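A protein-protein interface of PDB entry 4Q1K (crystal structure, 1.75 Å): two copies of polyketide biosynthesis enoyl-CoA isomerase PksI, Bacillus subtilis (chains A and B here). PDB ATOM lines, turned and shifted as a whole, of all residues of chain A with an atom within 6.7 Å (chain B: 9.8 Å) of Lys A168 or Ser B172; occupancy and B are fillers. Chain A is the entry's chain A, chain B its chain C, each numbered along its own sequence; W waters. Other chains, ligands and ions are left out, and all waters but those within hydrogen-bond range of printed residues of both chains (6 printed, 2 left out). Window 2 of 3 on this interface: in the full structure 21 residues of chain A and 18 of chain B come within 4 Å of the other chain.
The backbone carbonyl oxygen (O) of Leu A133 sits at hydrogen-bond distance from the side-chain amino group (NZ) of Lys A168, at 2.7 Å.
The backbone carbonyl oxygen (O) of Ala A135 is in hydrogen-bond range of the side-chain amino group (NZ) of Lys A168.
The backbone carbonyl oxygen (O) of Phe B171 sits close to the side-chain amide oxygen (OE1) of Gln B175, at 3.0 Å.
OE1 of Glu B176 is in salt-bridge range of NH2 of Arg B192.
NH2 of Arg B192 sits at hydrogen-bond distance from O of Pro A195 (2.9 Å).
Water W2 lies within hydrogen-bond range of the backbone carbonyl oxygen of Val A138 (2.6 Å) and the guanidinium group of Arg B192 (3.5 Å).
Water W1 lies within hydrogen-bond range of O of Asp A136 (2.6 Å), NZ of Lys A168 (3.0 Å) and OG of Ser B172 (3.2 Å).
Water W5 bridges O of Ser B172 (2.7 Å) and O of Asp A136 (2.8 Å).
Water W6 lies within hydrogen-bond range of OD1 of Asp A136 (2.7 Å) and NE2 of Gln B175 (2.9 Å).
Water W3 lies within hydrogen-bond range of O of Pro A195 (2.7 Å), OG of Ser B172 (2.8 Å) and N of Leu B173 (3.4 Å).
Water W4 bridges the side-chain amide nitrogen (NE2) of Gln B175 (2.8 Å) and the side-chain carboxylate (OD1) of Asp A136 (2.9 Å).
6 positions are printed for both chains.
Of the 9 pairs that touch across the chains among the printed residues, none has its exchanged pair printed and touching as well.
Lys A168 touches two residues of chain B.
No residue of chain B comes within 4 Å of Leu A169.
Of the printed residues of chain B, Val A194 touches Arg B192 (3.6 Å).
Pro A195 touches just these residues of chain B: Ser B172 (3.6 Å) and Arg B192 (2.9 Å).
Of the printed residues of chain B, Leu A234 touches Phe B171.
Leu B169 touches none of the printed residues of chain A.
Of the printed residues of chain A, Phe B171 touches Lys A167, Lys A168 and Leu A234.
Of chain A, only Lys A168 (3.9 Å), Pro A195 (3.6 Å) and Phe A196 (3.3 Å) come within 4 Å of Ser B172.
Of the printed residues of chain A, Gln B175 touches Asp A136.
Printed residues of chain A within 4 Å of Arg B192: Val A194 (3.6 Å) and Pro A195 (2.9 Å).
The nearest residue of chain B that does not touch Lys A168 is Gln B175 (5.5 Å).
The nearest residue of chain A that does not touch Ser B172 is Asp A136 (4.6 Å).
The nearest printed residue of chain A that does not touch Phe B171 is Asp A136 (5.9 Å).
Printed residues of chain B that touch a printed residue of chain A: Phe B171, Ser B172, Gln B175 and Arg B192.
Of the 19 printed residues of chain A, 7 touch a printed residue of chain B.
Printed residues of chain A that touch a printed residue of chain B: Asp A136, Lys A167, Lys A168, Val A194, Pro A195, Phe A196 and Leu A234.
Hydrophobic or aromatic side chains of chain A within 4 Å of the printed part of chain B: Pro A195, Phe A196 and Leu A234.
Among the printed residues, 9 pairs touch across the chains.
Among the printed residues, no Asp or Glu carboxylate lies within 4 Å of a Lys or Arg side-chain nitrogen of the other chain.
CB of Gln B175 touches O of Asp A136 (3.5 Å).
Lys A167 touches Phe B171.
Lys A168 touches Phe B171 (CE to CE2, 3.3 Å).
Ser B172 touches Lys A168 (CB to O, 3.9 Å).
Val A194 touches Arg B192 (O to O, 3.6 Å).
Pro A195 touches Ser B172.
Ser B172 touches Phe A196 (OG to CE1, 3.3 Å).
Leu A234 touches Phe B171 (CD1 to CZ, 3.6 Å).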
ATOM      1  N   GLY A 132       4.190  -1.392   8.277  1.00  0.00           N
ATOM      2  CA  GLY A 132       3.027  -0.914   8.996  1.00  0.00           C
ATOM      3  C   GLY A 132       2.472   0.405   8.447  1.00  0.00           C
ATOM      4  O   GLY A 132       1.269   0.597   8.396  1.00  0.00           O
ATOM      5  N   LEU A 133       3.389   1.340   8.094  1.00  0.00           N
ATOM      6  CA  LEU A 133       2.925   2.672   7.609  1.00  0.00           C
ATOM      7  C   LEU A 133       2.115   2.597   6.292  1.00  0.00           C
ATOM      8  O   LEU A 133       1.338   3.568   5.975  1.00  0.00           O
ATOM      9  CB  LEU A 133       4.129   3.571   7.380  1.00  0.00           C
ATOM     10  CG  LEU A 133       4.822   3.997   8.741  1.00  0.00           C
ATOM     11  CD1 LEU A 133       6.105   4.814   8.414  1.00  0.00           C
ATOM     12  CD2 LEU A 133       3.906   4.733   9.714  1.00  0.00           C
ATOM     13  N   PHE A 134       2.367   1.554   5.481  1.00  0.00           N
ATOM     14  CA  PHE A 134       1.593   1.382   4.252  1.00  0.00           C
ATOM     15  C   PHE A 134       0.156   0.946   4.549  1.00  0.00           C
ATOM     16  O   PHE A 134      -0.672   0.903   3.603  1.00  0.00           O
ATOM     17  CB  PHE A 134       2.245   0.373   3.288  1.00  0.00           C
ATOM     18  CG  PHE A 134       3.332   1.010   2.429  1.00  0.00           C
ATOM     19  CD1 PHE A 134       2.974   1.845   1.377  1.00  0.00           C
ATOM     20  CD2 PHE A 134       4.710   0.828   2.718  1.00  0.00           C
ATOM     21  CE1 PHE A 134       3.923   2.450   0.569  1.00  0.00           C
ATOM     22  CE2 PHE A 134       5.697   1.427   1.877  1.00  0.00           C
ATOM     23  CZ  PHE A 134       5.318   2.206   0.804  1.00  0.00           C
ATOM     24  N   ALA A 135      -0.152   0.604   5.804  1.00  0.00           N
ATOM     25  CA  ALA A 135      -1.560   0.293   6.113  1.00  0.00           C
ATOM     26  C   ALA A 135      -2.499   1.502   5.999  1.00  0.00           C
ATOM     27  O   ALA A 135      -2.054   2.626   6.085  1.00  0.00           O
ATOM     28  CB  ALA A 135      -1.697  -0.353   7.504  1.00  0.00           C
ATOM     29  N   ASP A 136      -3.817   1.251   5.895  1.00  0.00           N
ATOM     30  CA  ASP A 136      -4.766   2.392   5.787  1.00  0.00           C
ATOM     31  C   ASP A 136      -4.944   3.095   7.117  1.00  0.00           C
ATOM     32  O   ASP A 136      -5.181   4.330   7.160  1.00  0.00           O
ATOM     33  CB  ASP A 136      -6.084   1.827   5.290  1.00  0.00           C
ATOM     34  CG  ASP A 136      -5.847   1.132   3.927  1.00  0.00           C
ATOM     35  OD1 ASP A 136      -5.572   1.911   2.934  1.00  0.00           O
ATOM     36  OD2 ASP A 136      -5.785  -0.150   3.881  1.00  0.00           O
ATOM     37  N   ILE A 137      -4.948   2.304   8.181  1.00  0.00           N
ATOM     38  CA  ILE A 137      -5.057   2.915   9.560  1.00  0.00           C
ATOM     39  C   ILE A 137      -3.890   2.314  10.383  1.00  0.00           C
ATOM     40  O   ILE A 137      -3.681   1.090  10.368  1.00  0.00           O
ATOM     41  CB  ILE A 137      -6.409   2.513  10.168  1.00  0.00           C
ATOM     42  CG1 ILE A 137      -7.528   3.196   9.301  1.00  0.00           C
ATOM     43  CG2 ILE A 137      -6.485   2.954  11.644  1.00  0.00           C
ATOM     44  CD1 ILE A 137      -8.914   2.662   9.652  1.00  0.00           C
ATOM     45  N   VAL A 138      -3.185   3.193  11.091  1.00  0.00           N
ATOM     46  CA  VAL A 138      -1.943   2.783  11.832  1.00  0.00           C
ATOM     47  C   VAL A 138      -2.216   3.160  13.342  1.00  0.00           C
ATOM     48  O   VAL A 138      -2.699   4.262  13.645  1.00  0.00           O
ATOM     49  CB  VAL A 138      -0.715   3.532  11.365  1.00  0.00           C
ATOM     50  CG1 VAL A 138       0.502   3.085  12.206  1.00  0.00           C
ATOM     51  CG2 VAL A 138      -0.429   3.287   9.884  1.00  0.00           C
ATOM     52  N   PHE A 163       9.103   7.544   0.577  1.00  0.00           N
ATOM     53  CA  PHE A 163       7.792   7.967   0.117  1.00  0.00           C
ATOM     54  C   PHE A 163       6.749   7.905   1.267  1.00  0.00           C
ATOM     55  O   PHE A 163       5.999   8.858   1.468  1.00  0.00           O
ATOM     56  CB  PHE A 163       7.313   7.017  -1.039  1.00  0.00           C
ATOM     57  CG  PHE A 163       5.916   7.316  -1.520  1.00  0.00           C
ATOM     58  CD1 PHE A 163       5.689   8.487  -2.284  1.00  0.00           C
ATOM     59  CD2 PHE A 163       4.837   6.458  -1.197  1.00  0.00           C
ATOM     60  CE1 PHE A 163       4.383   8.818  -2.734  1.00  0.00           C
ATOM     61  CE2 PHE A 163       3.565   6.761  -1.683  1.00  0.00           C
ATOM     62  CZ  PHE A 163       3.356   7.967  -2.438  1.00  0.00           C
ATOM     63  N   ILE A 164       6.665   6.767   1.947  1.00  0.00           N
ATOM     64  CA  ILE A 164       5.523   6.532   2.842  1.00  0.00           C
ATOM     65  C   ILE A 164       5.667   7.311   4.158  1.00  0.00           C
ATOM     66  O   ILE A 164       4.719   7.692   4.766  1.00  0.00           O
ATOM     67  CB  ILE A 164       5.281   5.017   3.044  1.00  0.00           C
ATOM     68  CG1 ILE A 164       3.840   4.771   3.626  1.00  0.00           C
ATOM     69  CG2 ILE A 164       6.299   4.440   4.053  1.00  0.00           C
ATOM     70  CD1 ILE A 164       2.590   5.150   2.785  1.00  0.00           C
ATOM     71  N   VAL A 165       6.915   7.581   4.588  1.00  0.00           N
ATOM     72  CA  VAL A 165       7.085   8.316   5.874  1.00  0.00           C
ATOM     73  C   VAL A 165       6.604   9.762   5.698  1.00  0.00           C
ATOM     74  O   VAL A 165       5.830  10.198   6.461  1.00  0.00           O
ATOM     75  CB  VAL A 165       8.519   8.202   6.399  1.00  0.00           C
ATOM     76  CG1 VAL A 165       8.689   9.066   7.690  1.00  0.00           C
ATOM     77  CG2 VAL A 165       8.870   6.698   6.731  1.00  0.00           C
ATOM     78  N   PRO A 166       7.050  10.503   4.631  1.00  0.00           N
ATOM     79  CA  PRO A 166       6.476  11.823   4.456  1.00  0.00           C
ATOM     80  C   PRO A 166       4.961  11.753   4.195  1.00  0.00           C
ATOM     81  O   PRO A 166       4.222  12.637   4.640  1.00  0.00           O
ATOM     82  CB  PRO A 166       7.238  12.421   3.230  1.00  0.00           C
ATOM     83  CG  PRO A 166       8.454  11.544   3.083  1.00  0.00           C
ATOM     84  CD  PRO A 166       8.134  10.189   3.667  1.00  0.00           C
ATOM     85  N   LYS A 167       4.485  10.748   3.427  1.00  0.00           N
ATOM     86  CA  LYS A 167       3.057  10.676   3.115  1.00  0.00           C
ATOM     87  C   LYS A 167       2.189  10.518   4.410  1.00  0.00           C
ATOM     88  O   LYS A 167       1.158  11.182   4.552  1.00  0.00           O
ATOM     89  CB  LYS A 167       2.736   9.444   2.166  1.00  0.00           C
ATOM     90  CG  LYS A 167       1.230   9.396   1.791  1.00  0.00           C
ATOM     91  CD  LYS A 167       1.032  10.710   0.959  1.00  0.00           C
ATOM     92  CE  LYS A 167       0.795  10.585  -0.495  1.00  0.00           C
ATOM     93  NZ  LYS A 167       0.929  11.929  -1.154  1.00  0.00           N
ATOM     94  N   LYS A 168       2.655   9.752   5.364  1.00  0.00           N
ATOM     95  CA  LYS A 168       1.809   9.427   6.561  1.00  0.00           C
ATOM     96  C   LYS A 168       2.126  10.353   7.759  1.00  0.00           C
ATOM     97  O   LYS A 168       1.224  10.738   8.520  1.00  0.00           O
ATOM     98  CB  LYS A 168       2.088   7.983   6.974  1.00  0.00           C
ATOM     99  CG  LYS A 168       1.534   6.925   5.946  1.00  0.00           C
ATOM    100  CD  LYS A 168       0.012   7.205   5.648  1.00  0.00           C
ATOM    101  CE  LYS A 168      -0.498   6.193   4.642  1.00  0.00           C
ATOM    102  NZ  LYS A 168      -0.913   4.934   5.357  1.00  0.00           N
ATOM    103  N   LEU A 169       3.380  10.755   7.892  1.00  0.00           N
ATOM    104  CA  LEU A 169       3.811  11.563   9.087  1.00  0.00           C
ATOM    105  C   LEU A 169       4.152  13.012   8.719  1.00  0.00           C
ATOM    106  O   LEU A 169       4.389  13.844   9.611  1.00  0.00           O
ATOM    107  CB  LEU A 169       5.005  10.921   9.759  1.00  0.00           C
ATOM    108  CG  LEU A 169       4.671   9.562  10.364  1.00  0.00           C
ATOM    109  CD1 LEU A 169       5.893   9.210  11.169  1.00  0.00           C
ATOM    110  CD2 LEU A 169       3.569   9.763  11.402  1.00  0.00           C
ATOM    111  N   GLY A 170       4.032  13.351   7.424  1.00  0.00           N
ATOM    112  CA  GLY A 170       4.281  14.743   6.983  1.00  0.00           C
ATOM    113  C   GLY A 170       5.694  15.023   6.631  1.00  0.00           C
ATOM    114  O   GLY A 170       6.602  14.339   7.090  1.00  0.00           O
ATOM    115  N   VAL A 194       1.679  13.383  15.721  1.00  0.00           N
ATOM    116  CA  VAL A 194       1.249  12.390  14.648  1.00  0.00           C
ATOM    117  C   VAL A 194      -0.276  12.127  14.571  1.00  0.00           C
ATOM    118  O   VAL A 194      -0.987  12.235  15.560  1.00  0.00           O
ATOM    119  CB  VAL A 194       2.015  11.064  14.707  1.00  0.00           C
ATOM    120  CG1 VAL A 194       3.518  11.330  14.642  1.00  0.00           C
ATOM    121  CG2 VAL A 194       1.607  10.246  15.992  1.00  0.00           C
ATOM    122  N   PRO A 195      -0.790  11.791  13.379  1.00  0.00           N
ATOM    123  CA  PRO A 195      -2.250  11.601  13.147  1.00  0.00           C
ATOM    124  C   PRO A 195      -2.686  10.226  13.589  1.00  0.00           C
ATOM    125  O   PRO A 195      -3.861   9.946  13.538  1.00  0.00           O
ATOM    126  CB  PRO A 195      -2.398  11.737  11.607  1.00  0.00           C
ATOM    127  CG  PRO A 195      -1.048  11.359  11.057  1.00  0.00           C
ATOM    128  CD  PRO A 195      -0.017  11.841  12.106  1.00  0.00           C
ATOM    129  N   PHE A 196      -1.761   9.373  14.054  1.00  0.00           N
ATOM    130  CA  PHE A 196      -2.196   8.027  14.427  1.00  0.00           C
ATOM    131  C   PHE A 196      -2.677   8.031  15.863  1.00  0.00           C
ATOM    132  O   PHE A 196      -2.075   8.718  16.702  1.00  0.00           O
ATOM    133  CB  PHE A 196      -1.030   7.062  14.421  1.00  0.00           C
ATOM    134  CG  PHE A 196      -0.174   7.099  13.124  1.00  0.00           C
ATOM    135  CD1 PHE A 196      -0.772   7.303  11.876  1.00  0.00           C
ATOM    136  CD2 PHE A 196       1.214   6.911  13.172  1.00  0.00           C
ATOM    137  CE1 PHE A 196      -0.012   7.332  10.701  1.00  0.00           C
ATOM    138  CE2 PHE A 196       1.984   6.891  11.998  1.00  0.00           C
ATOM    139  CZ  PHE A 196       1.352   7.084  10.744  1.00  0.00           C
ATOM    140  N   LEU A 234      -0.749   6.681  -4.240  1.00  0.00           N
ATOM    141  CA  LEU A 234       0.346   5.928  -3.642  1.00  0.00           C
ATOM    142  C   LEU A 234       0.781   4.749  -4.531  1.00  0.00           C
ATOM    143  O   LEU A 234       1.973   4.514  -4.776  1.00  0.00           O
ATOM    144  CB  LEU A 234      -0.113   5.348  -2.251  1.00  0.00           C
ATOM    145  CG  LEU A 234      -0.088   6.392  -1.130  1.00  0.00           C
ATOM    146  CD1 LEU A 234      -1.142   7.451  -1.290  1.00  0.00           C
ATOM    147  CD2 LEU A 234      -0.342   5.698   0.195  1.00  0.00           C
ATOM    148  N   VAL B 165     -10.943  16.703   2.649  1.00  0.00           N
ATOM    149  CA  VAL B 165     -10.575  16.119   3.944  1.00  0.00           C
ATOM    150  C   VAL B 165      -9.021  15.816   4.061  1.00  0.00           C
ATOM    151  O   VAL B 165      -8.360  16.287   5.027  1.00  0.00           O
ATOM    152  CB  VAL B 165     -11.504  14.945   4.332  1.00  0.00           C
ATOM    153  CG1 VAL B 165     -11.026  14.308   5.699  1.00  0.00           C
ATOM    154  CG2 VAL B 165     -12.950  15.473   4.477  1.00  0.00           C
ATOM    155  N   PRO B 166      -8.427  15.089   3.086  1.00  0.00           N
ATOM    156  CA  PRO B 166      -6.962  14.927   3.146  1.00  0.00           C
ATOM    157  C   PRO B 166      -6.233  16.289   3.028  1.00  0.00           C
ATOM    158  O   PRO B 166      -5.171  16.539   3.680  1.00  0.00           O
ATOM    159  CB  PRO B 166      -6.660  14.073   1.892  1.00  0.00           C
ATOM    160  CG  PRO B 166      -7.938  13.351   1.580  1.00  0.00           C
ATOM    161  CD  PRO B 166      -9.062  14.242   2.024  1.00  0.00           C
ATOM    162  N   LYS B 167      -6.797  17.193   2.235  1.00  0.00           N
ATOM    163  CA  LYS B 167      -6.185  18.505   2.014  1.00  0.00           C
ATOM    164  C   LYS B 167      -6.090  19.376   3.275  1.00  0.00           C
ATOM    165  O   LYS B 167      -5.164  20.175   3.415  1.00  0.00           O
ATOM    166  CB  LYS B 167      -6.935  19.261   0.915  1.00  0.00           C
ATOM    167  CG  LYS B 167      -6.128  20.375   0.267  1.00  0.00           C
ATOM    168  CD  LYS B 167      -4.877  19.831  -0.404  1.00  0.00           C
ATOM    169  CE  LYS B 167      -3.953  20.954  -0.843  1.00  0.00           C
ATOM    170  NZ  LYS B 167      -2.885  20.468  -1.761  1.00  0.00           N
ATOM    171  N   LYS B 168      -7.051  19.220   4.180  1.00  0.00           N
ATOM    172  CA  LYS B 168      -7.143  20.066   5.425  1.00  0.00           C
ATOM    173  C   LYS B 168      -6.645  19.313   6.635  1.00  0.00           C
ATOM    174  O   LYS B 168      -5.997  19.910   7.547  1.00  0.00           O
ATOM    175  CB  LYS B 168      -8.581  20.607   5.658  1.00  0.00           C
ATOM    176  CG  LYS B 168      -9.051  21.550   4.500  1.00  0.00           C
ATOM    177  CD  LYS B 168      -8.127  22.758   4.536  1.00  0.00           C
ATOM    178  CE  LYS B 168      -8.524  23.677   3.419  1.00  0.00           C
ATOM    179  NZ  LYS B 168      -9.510  24.634   3.986  1.00  0.00           N
ATOM    180  N   LEU B 169      -6.953  18.019   6.677  1.00  0.00           N
ATOM    181  CA  LEU B 169      -6.666  17.229   7.890  1.00  0.00           C
ATOM    182  C   LEU B 169      -5.518  16.257   7.716  1.00  0.00           C
ATOM    183  O   LEU B 169      -5.131  15.596   8.703  1.00  0.00           O
ATOM    184  CB  LEU B 169      -7.939  16.499   8.387  1.00  0.00           C
ATOM    185  CG  LEU B 169      -9.086  17.423   8.745  1.00  0.00           C
ATOM    186  CD1 LEU B 169     -10.118  16.535   9.389  1.00  0.00           C
ATOM    187  CD2 LEU B 169      -8.530  18.494   9.712  1.00  0.00           C
ATOM    188  N   GLY B 170      -4.929  16.167   6.509  1.00  0.00           N
ATOM    189  CA  GLY B 170      -3.801  15.286   6.245  1.00  0.00           C
ATOM    190  C   GLY B 170      -4.280  13.914   5.736  1.00  0.00           C
ATOM    191  O   GLY B 170      -5.342  13.436   6.072  1.00  0.00           O
ATOM    192  N   PHE B 171      -3.424  13.278   4.942  1.00  0.00           N
ATOM    193  CA  PHE B 171      -3.720  11.987   4.324  1.00  0.00           C
ATOM    194  C   PHE B 171      -4.162  10.935   5.362  1.00  0.00           C
ATOM    195  O   PHE B 171      -5.218  10.229   5.176  1.00  0.00           O
ATOM    196  CB  PHE B 171      -2.506  11.486   3.597  1.00  0.00           C
ATOM    197  CG  PHE B 171      -2.772  10.169   2.881  1.00  0.00           C
ATOM    198  CD1 PHE B 171      -3.332  10.188   1.602  1.00  0.00           C
ATOM    199  CD2 PHE B 171      -2.521   8.941   3.514  1.00  0.00           C
ATOM    200  CE1 PHE B 171      -3.615   8.951   0.939  1.00  0.00           C
ATOM    201  CE2 PHE B 171      -2.864   7.731   2.867  1.00  0.00           C
ATOM    202  CZ  PHE B 171      -3.341   7.758   1.568  1.00  0.00           C
ATOM    203  N   SER B 172      -3.377  10.752   6.428  1.00  0.00           N
ATOM    204  CA  SER B 172      -3.625   9.652   7.337  1.00  0.00           C
ATOM    205  C   SER B 172      -4.972   9.752   8.120  1.00  0.00           C
ATOM    206  O   SER B 172      -5.828   8.830   8.082  1.00  0.00           O
ATOM    207  CB  SER B 172      -2.458   9.525   8.317  1.00  0.00           C
ATOM    208  OG  SER B 172      -2.701   8.353   9.119  1.00  0.00           O
ATOM    209  N   LEU B 173      -5.225  10.914   8.716  1.00  0.00           N
ATOM    210  CA  LEU B 173      -6.505  11.034   9.431  1.00  0.00           C
ATOM    211  C   LEU B 173      -7.748  10.966   8.463  1.00  0.00           C
ATOM    212  O   LEU B 173      -8.809  10.393   8.860  1.00  0.00           O
ATOM    213  CB  LEU B 173      -6.503  12.309  10.274  1.00  0.00           C
ATOM    214  CG  LEU B 173      -7.673  12.475  11.208  1.00  0.00           C
ATOM    215  CD1 LEU B 173      -7.640  11.329  12.286  1.00  0.00           C
ATOM    216  CD2 LEU B 173      -7.667  13.856  11.872  1.00  0.00           C
ATOM    217  N   ALA B 174      -7.588  11.518   7.235  1.00  0.00           N
ATOM    218  CA  ALA B 174      -8.606  11.486   6.225  1.00  0.00           C
ATOM    219  C   ALA B 174      -8.985  10.019   5.919  1.00  0.00           C
ATOM    220  O   ALA B 174     -10.208   9.702   5.756  1.00  0.00           O
ATOM    221  CB  ALA B 174      -8.111  12.183   4.928  1.00  0.00           C
ATOM    222  N   GLN B 175      -7.968   9.091   5.841  1.00  0.00           N
ATOM    223  CA  GLN B 175      -8.308   7.694   5.579  1.00  0.00           C
ATOM    224  C   GLN B 175      -9.357   7.157   6.604  1.00  0.00           C
ATOM    225  O   GLN B 175     -10.361   6.545   6.219  1.00  0.00           O
ATOM    226  CB  GLN B 175      -7.088   6.718   5.525  1.00  0.00           C
ATOM    227  CG  GLN B 175      -5.930   7.196   4.703  1.00  0.00           C
ATOM    228  CD  GLN B 175      -6.375   7.552   3.315  1.00  0.00           C
ATOM    229  OE1 GLN B 175      -6.499   8.755   2.949  1.00  0.00           O
ATOM    230  NE2 GLN B 175      -6.656   6.514   2.513  1.00  0.00           N
ATOM    231  N   GLU B 176      -9.099   7.342   7.898  1.00  0.00           N
ATOM    232  CA  GLU B 176      -9.981   6.881   8.956  1.00  0.00           C
ATOM    233  C   GLU B 176     -11.320   7.602   8.923  1.00  0.00           C
ATOM    234  O   GLU B 176     -12.382   6.982   8.951  1.00  0.00           O
ATOM    235  CB  GLU B 176      -9.247   7.170  10.305  1.00  0.00           C
ATOM    236  CG  GLU B 176     -10.044   6.719  11.492  1.00  0.00           C
ATOM    237  CD  GLU B 176      -9.343   7.200  12.769  1.00  0.00           C
ATOM    238  OE1 GLU B 176      -8.091   7.070  12.815  1.00  0.00           O
ATOM    239  OE2 GLU B 176     -10.061   7.800  13.616  1.00  0.00           O
ATOM    240  N   ILE B 177     -11.281   8.927   8.750  1.00  0.00           N
ATOM    241  CA  ILE B 177     -12.558   9.692   8.658  1.00  0.00           C
ATOM    242  C   ILE B 177     -13.449   9.238   7.501  1.00  0.00           C
ATOM    243  O   ILE B 177     -14.653   9.036   7.710  1.00  0.00           O
ATOM    244  CB  ILE B 177     -12.232  11.200   8.530  1.00  0.00           C
ATOM    245  CG1 ILE B 177     -11.688  11.659   9.912  1.00  0.00           C
ATOM    246  CG2 ILE B 177     -13.469  12.059   8.112  1.00  0.00           C
ATOM    247  CD1 ILE B 177     -11.133  13.072   9.860  1.00  0.00           C
ATOM    248  N   LEU B 178     -12.842   9.068   6.321  1.00  0.00           N
ATOM    249  CA  LEU B 178     -13.654   8.758   5.135  1.00  0.00           C
ATOM    250  C   LEU B 178     -14.068   7.288   5.087  1.00  0.00           C
ATOM    251  O   LEU B 178     -15.222   7.018   4.754  1.00  0.00           O
ATOM    252  CB  LEU B 178     -12.814   9.132   3.910  1.00  0.00           C
ATOM    253  CG  LEU B 178     -12.628  10.654   3.830  1.00  0.00           C
ATOM    254  CD1 LEU B 178     -11.616  10.868   2.737  1.00  0.00           C
ATOM    255  CD2 LEU B 178     -13.851  11.540   3.430  1.00  0.00           C
ATOM    256  N   LEU B 179     -13.154   6.348   5.371  1.00  0.00           N
ATOM    257  CA  LEU B 179     -13.513   4.912   5.230  1.00  0.00           C
ATOM    258  C   LEU B 179     -14.531   4.549   6.294  1.00  0.00           C
ATOM    259  O   LEU B 179     -15.470   3.713   6.069  1.00  0.00           O
ATOM    260  CB  LEU B 179     -12.255   3.963   5.381  1.00  0.00           C
ATOM    261  CG  LEU B 179     -11.244   4.075   4.207  1.00  0.00           C
ATOM    262  CD1 LEU B 179      -9.966   3.429   4.730  1.00  0.00           C
ATOM    263  CD2 LEU B 179     -11.898   3.169   3.171  1.00  0.00           C
ATOM    264  N   ASN B 180     -14.327   5.105   7.492  1.00  0.00           N
ATOM    265  CA  ASN B 180     -15.073   4.582   8.625  1.00  0.00           C
ATOM    266  C   ASN B 180     -16.315   5.404   9.002  1.00  0.00           C
ATOM    267  O   ASN B 180     -17.229   4.902   9.707  1.00  0.00           O
ATOM    268  CB  ASN B 180     -14.184   4.318   9.853  1.00  0.00           C
ATOM    269  CG  ASN B 180     -14.869   3.452  10.836  1.00  0.00           C
ATOM    270  OD1 ASN B 180     -15.498   2.470  10.445  1.00  0.00           O
ATOM    271  ND2 ASN B 180     -14.838   3.848  12.111  1.00  0.00           N
ATOM    272  N   TYR B 184     -16.824  12.292  15.678  1.00  0.00           N
ATOM    273  CA  TYR B 184     -15.748  12.792  16.528  1.00  0.00           C
ATOM    274  C   TYR B 184     -16.260  14.070  17.148  1.00  0.00           C
ATOM    275  O   TYR B 184     -16.656  14.988  16.459  1.00  0.00           O
ATOM    276  CB  TYR B 184     -14.485  13.171  15.740  1.00  0.00           C
ATOM    277  CG  TYR B 184     -13.870  12.023  14.932  1.00  0.00           C
ATOM    278  CD1 TYR B 184     -14.445  11.638  13.682  1.00  0.00           C
ATOM    279  CD2 TYR B 184     -12.787  11.331  15.403  1.00  0.00           C
ATOM    280  CE1 TYR B 184     -13.925  10.585  12.944  1.00  0.00           C
ATOM    281  CE2 TYR B 184     -12.228  10.286  14.657  1.00  0.00           C
ATOM    282  CZ  TYR B 184     -12.811   9.922  13.419  1.00  0.00           C
ATOM    283  OH  TYR B 184     -12.229   8.934  12.644  1.00  0.00           O
ATOM    284  N   ARG B 192      -6.485  14.381  18.513  1.00  0.00           N
ATOM    285  CA  ARG B 192      -5.801  13.651  17.384  1.00  0.00           C
ATOM    286  C   ARG B 192      -4.823  14.558  16.608  1.00  0.00           C
ATOM    287  O   ARG B 192      -4.053  14.118  15.764  1.00  0.00           O
ATOM    288  CB  ARG B 192      -6.818  12.990  16.434  1.00  0.00           C
ATOM    289  CG  ARG B 192      -7.759  11.989  17.089  1.00  0.00           C
ATOM    290  CD  ARG B 192      -7.027  10.676  17.490  1.00  0.00           C
ATOM    291  NE  ARG B 192      -6.348  10.064  16.319  1.00  0.00           N
ATOM    292  CZ  ARG B 192      -6.985   9.248  15.480  1.00  0.00           C
ATOM    293  NH1 ARG B 192      -8.295   8.987  15.714  1.00  0.00           N
ATOM    294  NH2 ARG B 192      -6.379   8.761  14.413  1.00  0.00           N
HETATM  295  O   HOH W   1      -3.134   5.968   7.093  1.00  0.00           O
HETATM  296  O   HOH W   2      -4.882   5.639  13.982  1.00  0.00           O
HETATM  297  O   HOH W   3      -4.510   8.734  11.192  1.00  0.00           O
HETATM  298  O   HOH W   4      -7.532   3.895   2.139  1.00  0.00           O
HETATM  299  O   HOH W   5      -5.880   6.347   9.011  1.00  0.00           O
HETATM  300  O   HOH W   6      -4.698   4.453   3.162  1.00  0.00           O
